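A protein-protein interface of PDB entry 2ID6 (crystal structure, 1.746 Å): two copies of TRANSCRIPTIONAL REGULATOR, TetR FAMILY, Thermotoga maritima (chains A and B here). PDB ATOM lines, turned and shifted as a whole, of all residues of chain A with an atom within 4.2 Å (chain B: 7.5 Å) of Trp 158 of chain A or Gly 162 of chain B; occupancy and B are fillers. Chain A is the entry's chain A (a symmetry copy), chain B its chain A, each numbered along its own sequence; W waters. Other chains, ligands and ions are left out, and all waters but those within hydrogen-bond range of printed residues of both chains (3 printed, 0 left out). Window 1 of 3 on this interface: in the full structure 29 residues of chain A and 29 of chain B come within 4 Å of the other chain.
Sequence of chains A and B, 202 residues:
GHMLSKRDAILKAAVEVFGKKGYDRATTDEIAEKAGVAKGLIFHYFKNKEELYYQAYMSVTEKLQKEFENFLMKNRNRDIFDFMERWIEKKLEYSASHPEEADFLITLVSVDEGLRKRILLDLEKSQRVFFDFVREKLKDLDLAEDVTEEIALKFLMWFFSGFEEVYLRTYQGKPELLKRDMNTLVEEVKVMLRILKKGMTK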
ATOM      1  N   LYS A 154      27.807   5.302  28.900  1.00  0.00           N
ATOM      2  CA  LYS A 154      27.700   6.612  28.240  1.00  0.00           C
ATOM      3  C   LYS A 154      28.283   7.728  29.115  1.00  0.00           C
ATOM      4  O   LYS A 154      29.120   8.561  28.651  1.00  0.00           O
ATOM      5  CB  LYS A 154      26.200   6.867  27.972  1.00  0.00           C
ATOM      6  CG  LYS A 154      25.888   8.021  27.098  1.00  0.00           C
ATOM      7  CD  LYS A 154      24.479   7.864  26.535  1.00  0.00           C
ATOM      8  CE  LYS A 154      24.402   6.681  25.574  1.00  0.00           C
ATOM      9  NZ  LYS A 154      23.039   6.108  25.496  1.00  0.00           N
ATOM     10  N   PHE A 155      27.877   7.721  30.385  1.00  0.00           N
ATOM     11  CA  PHE A 155      28.271   8.774  31.316  1.00  0.00           C
ATOM     12  C   PHE A 155      29.770   8.687  31.584  1.00  0.00           C
ATOM     13  O   PHE A 155      30.464   9.696  31.574  1.00  0.00           O
ATOM     14  CB  PHE A 155      27.467   8.633  32.615  1.00  0.00           C
ATOM     15  CG  PHE A 155      27.289   9.926  33.393  1.00  0.00           C
ATOM     16  CD1 PHE A 155      28.023  11.078  33.086  1.00  0.00           C
ATOM     17  CD2 PHE A 155      26.411   9.957  34.476  1.00  0.00           C
ATOM     18  CE1 PHE A 155      27.859  12.278  33.861  1.00  0.00           C
ATOM     19  CE2 PHE A 155      26.223  11.121  35.229  1.00  0.00           C
ATOM     20  CZ  PHE A 155      26.950  12.281  34.927  1.00  0.00           C
ATOM     21  N   LEU A 156      30.289   7.474  31.828  1.00  0.00           N
ATOM     22  CA  LEU A 156      31.718   7.350  32.108  1.00  0.00           C
ATOM     23  C   LEU A 156      32.585   7.735  30.905  1.00  0.00           C
ATOM     24  O   LEU A 156      33.654   8.341  31.058  1.00  0.00           O
ATOM     25  CB  LEU A 156      32.062   5.923  32.515  1.00  0.00           C
ATOM     26  CG  LEU A 156      31.613   5.566  33.925  1.00  0.00           C
ATOM     27  CD1 LEU A 156      32.036   4.125  34.169  1.00  0.00           C
ATOM     28  CD2 LEU A 156      32.254   6.484  34.953  1.00  0.00           C
ATOM     29  N   MET A 157      32.127   7.375  29.710  1.00  0.00           N
ATOM     30  CA  MET A 157      32.913   7.666  28.505  1.00  0.00           C
ATOM     31  C   MET A 157      32.899   9.165  28.190  1.00  0.00           C
ATOM     32  O   MET A 157      33.896   9.724  27.767  1.00  0.00           O
ATOM     33  CB  MET A 157      32.424   6.841  27.330  1.00  0.00           C
ATOM     34  CG  MET A 157      32.732   5.328  27.432  1.00  0.00           C
ATOM     35  SD  MET A 157      34.644   4.961  27.609  1.00  0.00           S
ATOM     36  CE  MET A 157      35.316   6.000  26.098  1.00  0.00           C
ATOM     37  N   TRP A 158      31.774   9.805  28.450  1.00  0.00           N
ATOM     38  CA  TRP A 158      31.674  11.272  28.349  1.00  0.00           C
ATOM     39  C   TRP A 158      32.576  11.944  29.378  1.00  0.00           C
ATOM     40  O   TRP A 158      33.269  12.894  29.059  1.00  0.00           O
ATOM     41  CB  TRP A 158      30.232  11.686  28.583  1.00  0.00           C
ATOM     42  CG  TRP A 158      29.965  13.154  28.533  1.00  0.00           C
ATOM     43  CD1 TRP A 158      30.690  14.123  27.897  1.00  0.00           C
ATOM     44  CD2 TRP A 158      28.830  13.801  29.085  1.00  0.00           C
ATOM     45  NE1 TRP A 158      30.103  15.356  28.081  1.00  0.00           N
ATOM     46  CE2 TRP A 158      28.946  15.184  28.790  1.00  0.00           C
ATOM     47  CE3 TRP A 158      27.729  13.351  29.809  1.00  0.00           C
ATOM     48  CZ2 TRP A 158      28.002  16.112  29.207  1.00  0.00           C
ATOM     49  CZ3 TRP A 158      26.794  14.271  30.220  1.00  0.00           C
ATOM     50  CH2 TRP A 158      26.937  15.646  29.917  1.00  0.00           C
ATOM     51  N   PHE A 159      32.562  11.466  30.621  1.00  0.00           N
ATOM     52  CA  PHE A 159      33.418  12.076  31.631  1.00  0.00           C
ATOM     53  C   PHE A 159      34.890  11.992  31.197  1.00  0.00           C
ATOM     54  O   PHE A 159      35.616  13.002  31.187  1.00  0.00           O
ATOM     55  CB  PHE A 159      33.223  11.383  32.987  1.00  0.00           C
ATOM     56  CG  PHE A 159      34.124  11.913  34.057  1.00  0.00           C
ATOM     57  CD1 PHE A 159      33.775  13.045  34.764  1.00  0.00           C
ATOM     58  CD2 PHE A 159      35.340  11.300  34.325  1.00  0.00           C
ATOM     59  CE1 PHE A 159      34.626  13.554  35.762  1.00  0.00           C
ATOM     60  CE2 PHE A 159      36.196  11.814  35.326  1.00  0.00           C
ATOM     61  CZ  PHE A 159      35.823  12.935  36.026  1.00  0.00           C
ATOM     62  N   PHE A 160      35.304  10.800  30.791  1.00  0.00           N
ATOM     63  CA  PHE A 160      36.685  10.586  30.452  1.00  0.00           C
ATOM     64  C   PHE A 160      37.068  11.457  29.243  1.00  0.00           C
ATOM     65  O   PHE A 160      38.016  12.234  29.314  1.00  0.00           O
ATOM     66  CB  PHE A 160      36.959   9.127  30.175  1.00  0.00           C
ATOM     67  CG  PHE A 160      38.318   8.900  29.559  1.00  0.00           C
ATOM     68  CD1 PHE A 160      39.464   8.960  30.362  1.00  0.00           C
ATOM     69  CD2 PHE A 160      38.452   8.705  28.182  1.00  0.00           C
ATOM     70  CE1 PHE A 160      40.729   8.794  29.803  1.00  0.00           C
ATOM     71  CE2 PHE A 160      39.728   8.531  27.609  1.00  0.00           C
ATOM     72  CZ  PHE A 160      40.853   8.577  28.427  1.00  0.00           C
ATOM     73  N   SER A 161      36.313  11.356  28.150  1.00  0.00           N
ATOM     74  CA  SER A 161      36.658  12.075  26.911  1.00  0.00           C
ATOM     75  C   SER A 161      36.409  13.593  26.993  1.00  0.00           C
ATOM     76  O   SER A 161      37.164  14.392  26.415  1.00  0.00           O
ATOM     77  CB  SER A 161      35.873  11.483  25.744  1.00  0.00           C
ATOM     78  OG  SER A 161      34.491  11.749  25.913  1.00  0.00           O
ATOM     79  N   GLY A 162      35.369  13.991  27.731  1.00  0.00           N
ATOM     80  CA  GLY A 162      35.086  15.392  27.969  1.00  0.00           C
ATOM     81  C   GLY A 162      36.145  16.058  28.841  1.00  0.00           C
ATOM     82  O   GLY A 162      36.516  17.197  28.569  1.00  0.00           O
ATOM     83  N   ILE B  88      17.608  22.133  30.216  1.00  0.00           N
ATOM     84  CA  ILE B  88      18.149  21.265  29.155  1.00  0.00           C
ATOM     85  C   ILE B  88      17.065  20.821  28.142  1.00  0.00           C
ATOM     86  O   ILE B  88      17.298  20.875  26.922  1.00  0.00           O
ATOM     87  CB  ILE B  88      18.966  20.077  29.740  1.00  0.00           C
ATOM     88  CG1 ILE B  88      20.239  20.594  30.423  1.00  0.00           C
ATOM     89  CG2 ILE B  88      19.347  19.057  28.659  1.00  0.00           C
ATOM     90  CD1 ILE B  88      20.937  19.532  31.326  1.00  0.00           C
ATOM     91  N   LEU B 156      28.870  20.414  38.020  1.00  0.00           N
ATOM     92  CA  LEU B 156      27.560  20.696  37.437  1.00  0.00           C
ATOM     93  C   LEU B 156      27.654  21.587  36.193  1.00  0.00           C
ATOM     94  O   LEU B 156      26.906  21.408  35.223  1.00  0.00           O
ATOM     95  CB  LEU B 156      26.656  21.380  38.455  1.00  0.00           C
ATOM     96  CG  LEU B 156      26.130  20.440  39.530  1.00  0.00           C
ATOM     97  CD1 LEU B 156      25.249  21.275  40.450  1.00  0.00           C
ATOM     98  CD2 LEU B 156      25.324  19.305  38.919  1.00  0.00           C
ATOM     99  N   MET B 157      28.568  22.552  36.228  1.00  0.00           N
ATOM    100  CA  MET B 157      28.698  23.479  35.098  1.00  0.00           C
ATOM    101  C   MET B 157      29.314  22.779  33.883  1.00  0.00           C
ATOM    102  O   MET B 157      28.926  23.029  32.755  1.00  0.00           O
ATOM    103  CB  MET B 157      29.493  24.708  35.498  1.00  0.00           C
ATOM    104  CG  MET B 157      28.760  25.659  36.477  1.00  0.00           C
ATOM    105  SD  MET B 157      27.059  26.304  35.763  1.00  0.00           S
ATOM    106  CE  MET B 157      27.662  26.960  34.025  1.00  0.00           C
ATOM    107  N   TRP B 158      30.236  21.869  34.139  1.00  0.00           N
ATOM    108  CA  TRP B 158      30.792  21.007  33.081  1.00  0.00           C
ATOM    109  C   TRP B 158      29.711  20.098  32.506  1.00  0.00           C
ATOM    110  O   TRP B 158      29.617  19.943  31.301  1.00  0.00           O
ATOM    111  CB  TRP B 158      31.911  20.166  33.666  1.00  0.00           C
ATOM    112  CG  TRP B 158      32.570  19.218  32.719  1.00  0.00           C
ATOM    113  CD1 TRP B 158      32.631  19.292  31.356  1.00  0.00           C
ATOM    114  CD2 TRP B 158      33.341  18.088  33.093  1.00  0.00           C
ATOM    115  NE1 TRP B 158      33.344  18.226  30.851  1.00  0.00           N
ATOM    116  CE2 TRP B 158      33.810  17.481  31.899  1.00  0.00           C
ATOM    117  CE3 TRP B 158      33.676  17.520  34.320  1.00  0.00           C
ATOM    118  CZ2 TRP B 158      34.588  16.332  31.908  1.00  0.00           C
ATOM    119  CZ3 TRP B 158      34.447  16.382  34.327  1.00  0.00           C
ATOM    120  CH2 TRP B 158      34.897  15.795  33.121  1.00  0.00           C
ATOM    121  N   PHE B 159      28.900  19.481  33.363  1.00  0.00           N
ATOM    122  CA  PHE B 159      27.848  18.611  32.852  1.00  0.00           C
ATOM    123  C   PHE B 159      26.910  19.403  31.929  1.00  0.00           C
ATOM    124  O   PHE B 159      26.636  18.994  30.786  1.00  0.00           O
ATOM    125  CB  PHE B 159      27.055  17.991  34.011  1.00  0.00           C
ATOM    126  CG  PHE B 159      25.912  17.139  33.558  1.00  0.00           C
ATOM    127  CD1 PHE B 159      26.121  15.822  33.206  1.00  0.00           C
ATOM    128  CD2 PHE B 159      24.636  17.672  33.445  1.00  0.00           C
ATOM    129  CE1 PHE B 159      25.051  15.022  32.768  1.00  0.00           C
ATOM    130  CE2 PHE B 159      23.562  16.868  33.000  1.00  0.00           C
ATOM    131  CZ  PHE B 159      23.790  15.555  32.667  1.00  0.00           C
ATOM    132  N   PHE B 160      26.467  20.556  32.409  1.00  0.00           N
ATOM    133  CA  PHE B 160      25.510  21.333  31.668  1.00  0.00           C
ATOM    134  C   PHE B 160      26.125  21.788  30.334  1.00  0.00           C
ATOM    135  O   PHE B 160      25.566  21.528  29.272  1.00  0.00           O
ATOM    136  CB  PHE B 160      25.028  22.516  32.473  1.00  0.00           C
ATOM    137  CG  PHE B 160      24.237  23.497  31.643  1.00  0.00           C
ATOM    138  CD1 PHE B 160      22.914  23.203  31.291  1.00  0.00           C
ATOM    139  CD2 PHE B 160      24.834  24.664  31.158  1.00  0.00           C
ATOM    140  CE1 PHE B 160      22.183  24.077  30.491  1.00  0.00           C
ATOM    141  CE2 PHE B 160      24.100  25.557  30.352  1.00  0.00           C
ATOM    142  CZ  PHE B 160      22.781  25.254  30.028  1.00  0.00           C
ATOM    143  N   SER B 161      27.289  22.433  30.384  1.00  0.00           N
ATOM    144  CA  SER B 161      27.908  22.994  29.170  1.00  0.00           C
ATOM    145  C   SER B 161      28.494  21.924  28.230  1.00  0.00           C
ATOM    146  O   SER B 161      28.451  22.069  26.997  1.00  0.00           O
ATOM    147  CB  SER B 161      28.996  23.988  29.566  1.00  0.00           C
ATOM    148  OG  SER B 161      30.063  23.303  30.200  1.00  0.00           O
ATOM    149  N   GLY B 162      29.018  20.839  28.809  1.00  0.00           N
ATOM    150  CA  GLY B 162      29.511  19.717  28.035  1.00  0.00           C
ATOM    151  C   GLY B 162      28.391  18.972  27.315  1.00  0.00           C
ATOM    152  O   GLY B 162      28.578  18.573  26.169  1.00  0.00           O
ATOM    153  N   PHE B 163      27.239  18.781  27.969  1.00  0.00           N
ATOM    154  CA  PHE B 163      26.104  18.066  27.348  1.00  0.00           C
ATOM    155  C   PHE B 163      25.677  18.816  26.090  1.00  0.00           C
ATOM    156  O   PHE B 163      25.459  18.226  25.017  1.00  0.00           O
ATOM    157  CB  PHE B 163      24.916  17.922  28.329  1.00  0.00           C
ATOM    158  CG  PHE B 163      23.704  17.206  27.733  1.00  0.00           C
ATOM    159  CD1 PHE B 163      23.637  15.819  27.745  1.00  0.00           C
ATOM    160  CD2 PHE B 163      22.642  17.924  27.168  1.00  0.00           C
ATOM    161  CE1 PHE B 163      22.527  15.140  27.191  1.00  0.00           C
ATOM    162  CE2 PHE B 163      21.549  17.270  26.624  1.00  0.00           C
ATOM    163  CZ  PHE B 163      21.491  15.867  26.646  1.00  0.00           C
ATOM    164  N   GLU B 164      25.581  20.124  26.233  1.00  0.00           N
ATOM    165  CA  GLU B 164      25.229  20.990  25.121  1.00  0.00           C
ATOM    166  C   GLU B 164      26.234  20.882  23.990  1.00  0.00           C
ATOM    167  O   GLU B 164      25.846  20.715  22.824  1.00  0.00           O
ATOM    168  CB  GLU B 164      25.127  22.435  25.595  1.00  0.00           C
ATOM    169  CG  GLU B 164      24.754  23.393  24.482  1.00  0.00           C
ATOM    170  CD  GLU B 164      24.698  24.835  24.940  1.00  0.00           C
ATOM    171  OE1 GLU B 164      25.465  25.211  25.853  1.00  0.00           O
ATOM    172  OE2 GLU B 164      23.899  25.594  24.353  1.00  0.00           O
ATOM    173  N   GLU B 165      27.518  20.955  24.309  1.00  0.00           N
ATOM    174  CA  GLU B 165      28.529  20.882  23.254  1.00  0.00           C
ATOM    175  C   GLU B 165      28.448  19.529  22.552  1.00  0.00           C
ATOM    176  O   GLU B 165      28.459  19.461  21.315  1.00  0.00           O
ATOM    177  CB  GLU B 165      29.938  21.171  23.760  1.00  0.00           C
ATOM    178  CG  GLU B 165      30.843  21.662  22.613  1.00  0.00           C
ATOM    179  CD  GLU B 165      32.315  21.657  22.966  1.00  0.00           C
ATOM    180  OE1 GLU B 165      32.649  21.642  24.176  1.00  0.00           O
ATOM    181  OE2 GLU B 165      33.137  21.649  22.024  1.00  0.00           O
ATOM    182  N   VAL B 166      28.290  18.448  23.331  1.00  0.00           N
ATOM    183  CA  VAL B 166      28.172  17.132  22.695  1.00  0.00           C
ATOM    184  C   VAL B 166      26.959  17.011  21.778  1.00  0.00           C
ATOM    185  O   VAL B 166      27.095  16.516  20.666  1.00  0.00           O
ATOM    186  CB  VAL B 166      28.177  15.981  23.729  1.00  0.00           C
ATOM    187  CG1 VAL B 166      27.939  14.640  23.047  1.00  0.00           C
ATOM    188  CG2 VAL B 166      29.495  15.955  24.409  1.00  0.00           C
ATOM    189  N   TYR B 167      25.775  17.433  22.214  1.00  0.00           N
ATOM    190  CA  TYR B 167      24.624  17.197  21.335  1.00  0.00           C
ATOM    191  C   TYR B 167      24.656  18.138  20.113  1.00  0.00           C
ATOM    192  O   TYR B 167      24.287  17.729  19.017  1.00  0.00           O
ATOM    193  CB  TYR B 167      23.269  17.173  22.073  1.00  0.00           C
ATOM    194  CG  TYR B 167      22.629  18.512  22.376  1.00  0.00           C
ATOM    195  CD1 TYR B 167      22.090  19.308  21.359  1.00  0.00           C
ATOM    196  CD2 TYR B 167      22.524  18.967  23.704  1.00  0.00           C
ATOM    197  CE1 TYR B 167      21.493  20.547  21.637  1.00  0.00           C
ATOM    198  CE2 TYR B 167      21.917  20.207  23.992  1.00  0.00           C
ATOM    199  CZ  TYR B 167      21.414  20.978  22.961  1.00  0.00           C
ATOM    200  OH  TYR B 167      20.813  22.191  23.239  1.00  0.00           O
ATOM    201  N   LEU B 168      25.186  19.349  20.275  1.00  0.00           N
ATOM    202  CA  LEU B 168      25.244  20.274  19.115  1.00  0.00           C
ATOM    203  C   LEU B 168      26.187  19.754  18.044  1.00  0.00           C
ATOM    204  O   LEU B 168      25.927  19.886  16.828  1.00  0.00           O
ATOM    205  CB  LEU B 168      25.639  21.697  19.537  1.00  0.00           C
ATOM    206  CG  LEU B 168      24.540  22.415  20.316  1.00  0.00           C
ATOM    207  CD1 LEU B 168      25.059  23.720  20.938  1.00  0.00           C
ATOM    208  CD2 LEU B 168      23.277  22.638  19.453  1.00  0.00           C
ATOM    209  N   ARG B 169      27.273  19.153  18.507  1.00  0.00           N
ATOM    210  CA  ARG B 169      28.282  18.602  17.613  1.00  0.00           C
ATOM    211  C   ARG B 169      27.792  17.322  16.979  1.00  0.00           C
ATOM    212  O   ARG B 169      27.936  17.139  15.778  1.00  0.00           O
ATOM    213  CB  ARG B 169      29.608  18.405  18.357  1.00  0.00           C
ATOM    214  CG  ARG B 169      30.309  19.746  18.504  1.00  0.00           C
ATOM    215  CD  ARG B 169      31.219  19.831  19.692  1.00  0.00           C
ATOM    216  NE  ARG B 169      32.624  19.644  19.374  1.00  0.00           N
ATOM    217  CZ  ARG B 169      33.537  19.244  20.264  1.00  0.00           C
ATOM    218  NH1 ARG B 169      33.199  18.976  21.524  1.00  0.00           N
ATOM    219  NH2 ARG B 169      34.798  19.102  19.897  1.00  0.00           N
ATOM    220  N   VAL B 189      19.367  12.279  30.282  1.00  0.00           N
ATOM    221  CA  VAL B 189      19.680  13.459  31.098  1.00  0.00           C
ATOM    222  C   VAL B 189      19.119  13.342  32.516  1.00  0.00           C
ATOM    223  O   VAL B 189      19.827  13.605  33.501  1.00  0.00           O
ATOM    224  CB  VAL B 189      19.106  14.717  30.432  1.00  0.00           C
ATOM    225  CG1 VAL B 189      19.048  15.900  31.410  1.00  0.00           C
ATOM    226  CG2 VAL B 189      19.938  15.048  29.246  1.00  0.00           C
ATOM    227  N   MET B 192      21.224  10.789  34.422  1.00  0.00           N
ATOM    228  CA  MET B 192      22.540  11.327  34.725  1.00  0.00           C
ATOM    229  C   MET B 192      22.483  12.391  35.824  1.00  0.00           C
ATOM    230  O   MET B 192      23.337  12.408  36.713  1.00  0.00           O
ATOM    231  CB  MET B 192      23.192  11.854  33.434  1.00  0.00           C
ATOM    232  CG  MET B 192      23.364  10.693  32.522  1.00  0.00           C
ATOM    233  SD  MET B 192      24.465  11.185  30.962  1.00  0.00           S
ATOM    234  CE  MET B 192      24.058   9.594  29.938  1.00  0.00           C
ATOM    235  N   LEU B 196      24.333  12.341  39.458  1.00  0.00           N
ATOM    236  CA  LEU B 196      25.102  13.436  40.065  1.00  0.00           C
ATOM    237  C   LEU B 196      24.590  13.889  41.415  1.00  0.00           C
ATOM    238  O   LEU B 196      25.377  14.068  42.341  1.00  0.00           O
ATOM    239  CB  LEU B 196      25.157  14.639  39.126  1.00  0.00           C
ATOM    240  CG  LEU B 196      26.028  14.466  37.919  1.00  0.00           C
ATOM    241  CD1 LEU B 196      25.870  15.766  37.157  1.00  0.00           C
ATOM    242  CD2 LEU B 196      27.500  14.259  38.312  1.00  0.00           C
HETATM  243  O   HOH W   1      31.825  17.337  26.445  1.00  0.00           O
HETATM  244  O   HOH W   2      31.210  16.110  30.772  1.00  0.00           O
HETATM  245  O   HOH W   3      33.464  18.692  27.796  1.00  0.00           O
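Trp 158 of chain A touches Phe 159 of chain B, and with the chains exchanged Phe 159 of chain A touches Trp 158 of chain B.
Trp 158 of chain A touches Gly 162 of chain B, and with the chains exchanged Gly 162 of chain A touches Trp 158 of chain B.
Positions printed for both chains: 156, 157, 158, 159, 160, 161 and 162.
Printed residues of chain B within 4 Å of Phe 155 of chain A: Phe 159 (3.97 Å), Met 192 (3.5 Å) and Leu 196 (3.8 Å).
Trp 158 of chain A touches just these residues of chain B: Phe 159, Gly 162, Phe 163, Val 166 and Met 192.
Printed residues of chain B within 4 Å of Phe 159 of chain A: Trp 158.
Gly 162 of chain B touches just one residue of chain A: Trp 158.
Of the printed residues of chain A, Phe 163 of chain B touches Trp 158.
Printed residues of chain A within 4 Å of Val 166 of chain B: Trp 158 (3.8 Å).
Printed residues of chain A within 4 Å of Met 192 of chain B: Lys 154, Phe 155 and Trp 158.
The nearest printed residue of chain A that does not touch Gly 162 of chain B is Gly 162 of chain A (7.1 Å).
The nearest printed residue of chain B that does not touch Gly 162 of chain A is Val 166 of chain B (6.7 Å).
Hydrophobic or aromatic side chains of chain A that line the printed part of chain B: Phe 155, Trp 158 and Phe 159.
Among the printed residues, no Asp or Glu carboxylate lies within 4 Å of a Lys or Arg side-chain nitrogen of the other chain.
Water W2 bridges NE1 of Trp 158 of chain A and NE1 of Trp 158 of chain B.
Water W1 lies within hydrogen-bond range of the indole nitrogen of Trp 158 of chain A (3.1 Å) and the backbone carbonyl oxygen of Gly 162 of chain B (3.5 Å).
Water W3 lies within hydrogen-bond range of the indole nitrogen (NE1) of Trp 158 of chain B and the backbone carbonyl oxygen (O) of Gly 162 of chain A.
Met 192 of chain B touches Lys 154 of chain A (CE to CG, 3.7 Å).
Phe 155 of chain A touches Phe 159 of chain B.
O of Met 192 of chain B touches CE2 of Phe 155 of chain A, at 3.5 Å.
Leu 196 of chain B touches Phe 155 of chain A.
Trp 158 of chain A touches Phe 159 of chain B (CZ3 to CE1, 3.2 Å).
CZ2 of Trp 158 of chain A touches N of Phe 163 of chain B, at 3.0 Å.
Trp 158 of chain A touches Val 166 of chain B (NE1 to CG2, 3.8 Å).
Trp 158 of chain A touches Met 192 of chain B.
Phe 159 of chain A touches Trp 158 of chain B (CE1 to CZ3, 3.2 Å).
CZ2 of Trp 158 of chain B touches C of Gly 162 of chain A, 3.5 Å away.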
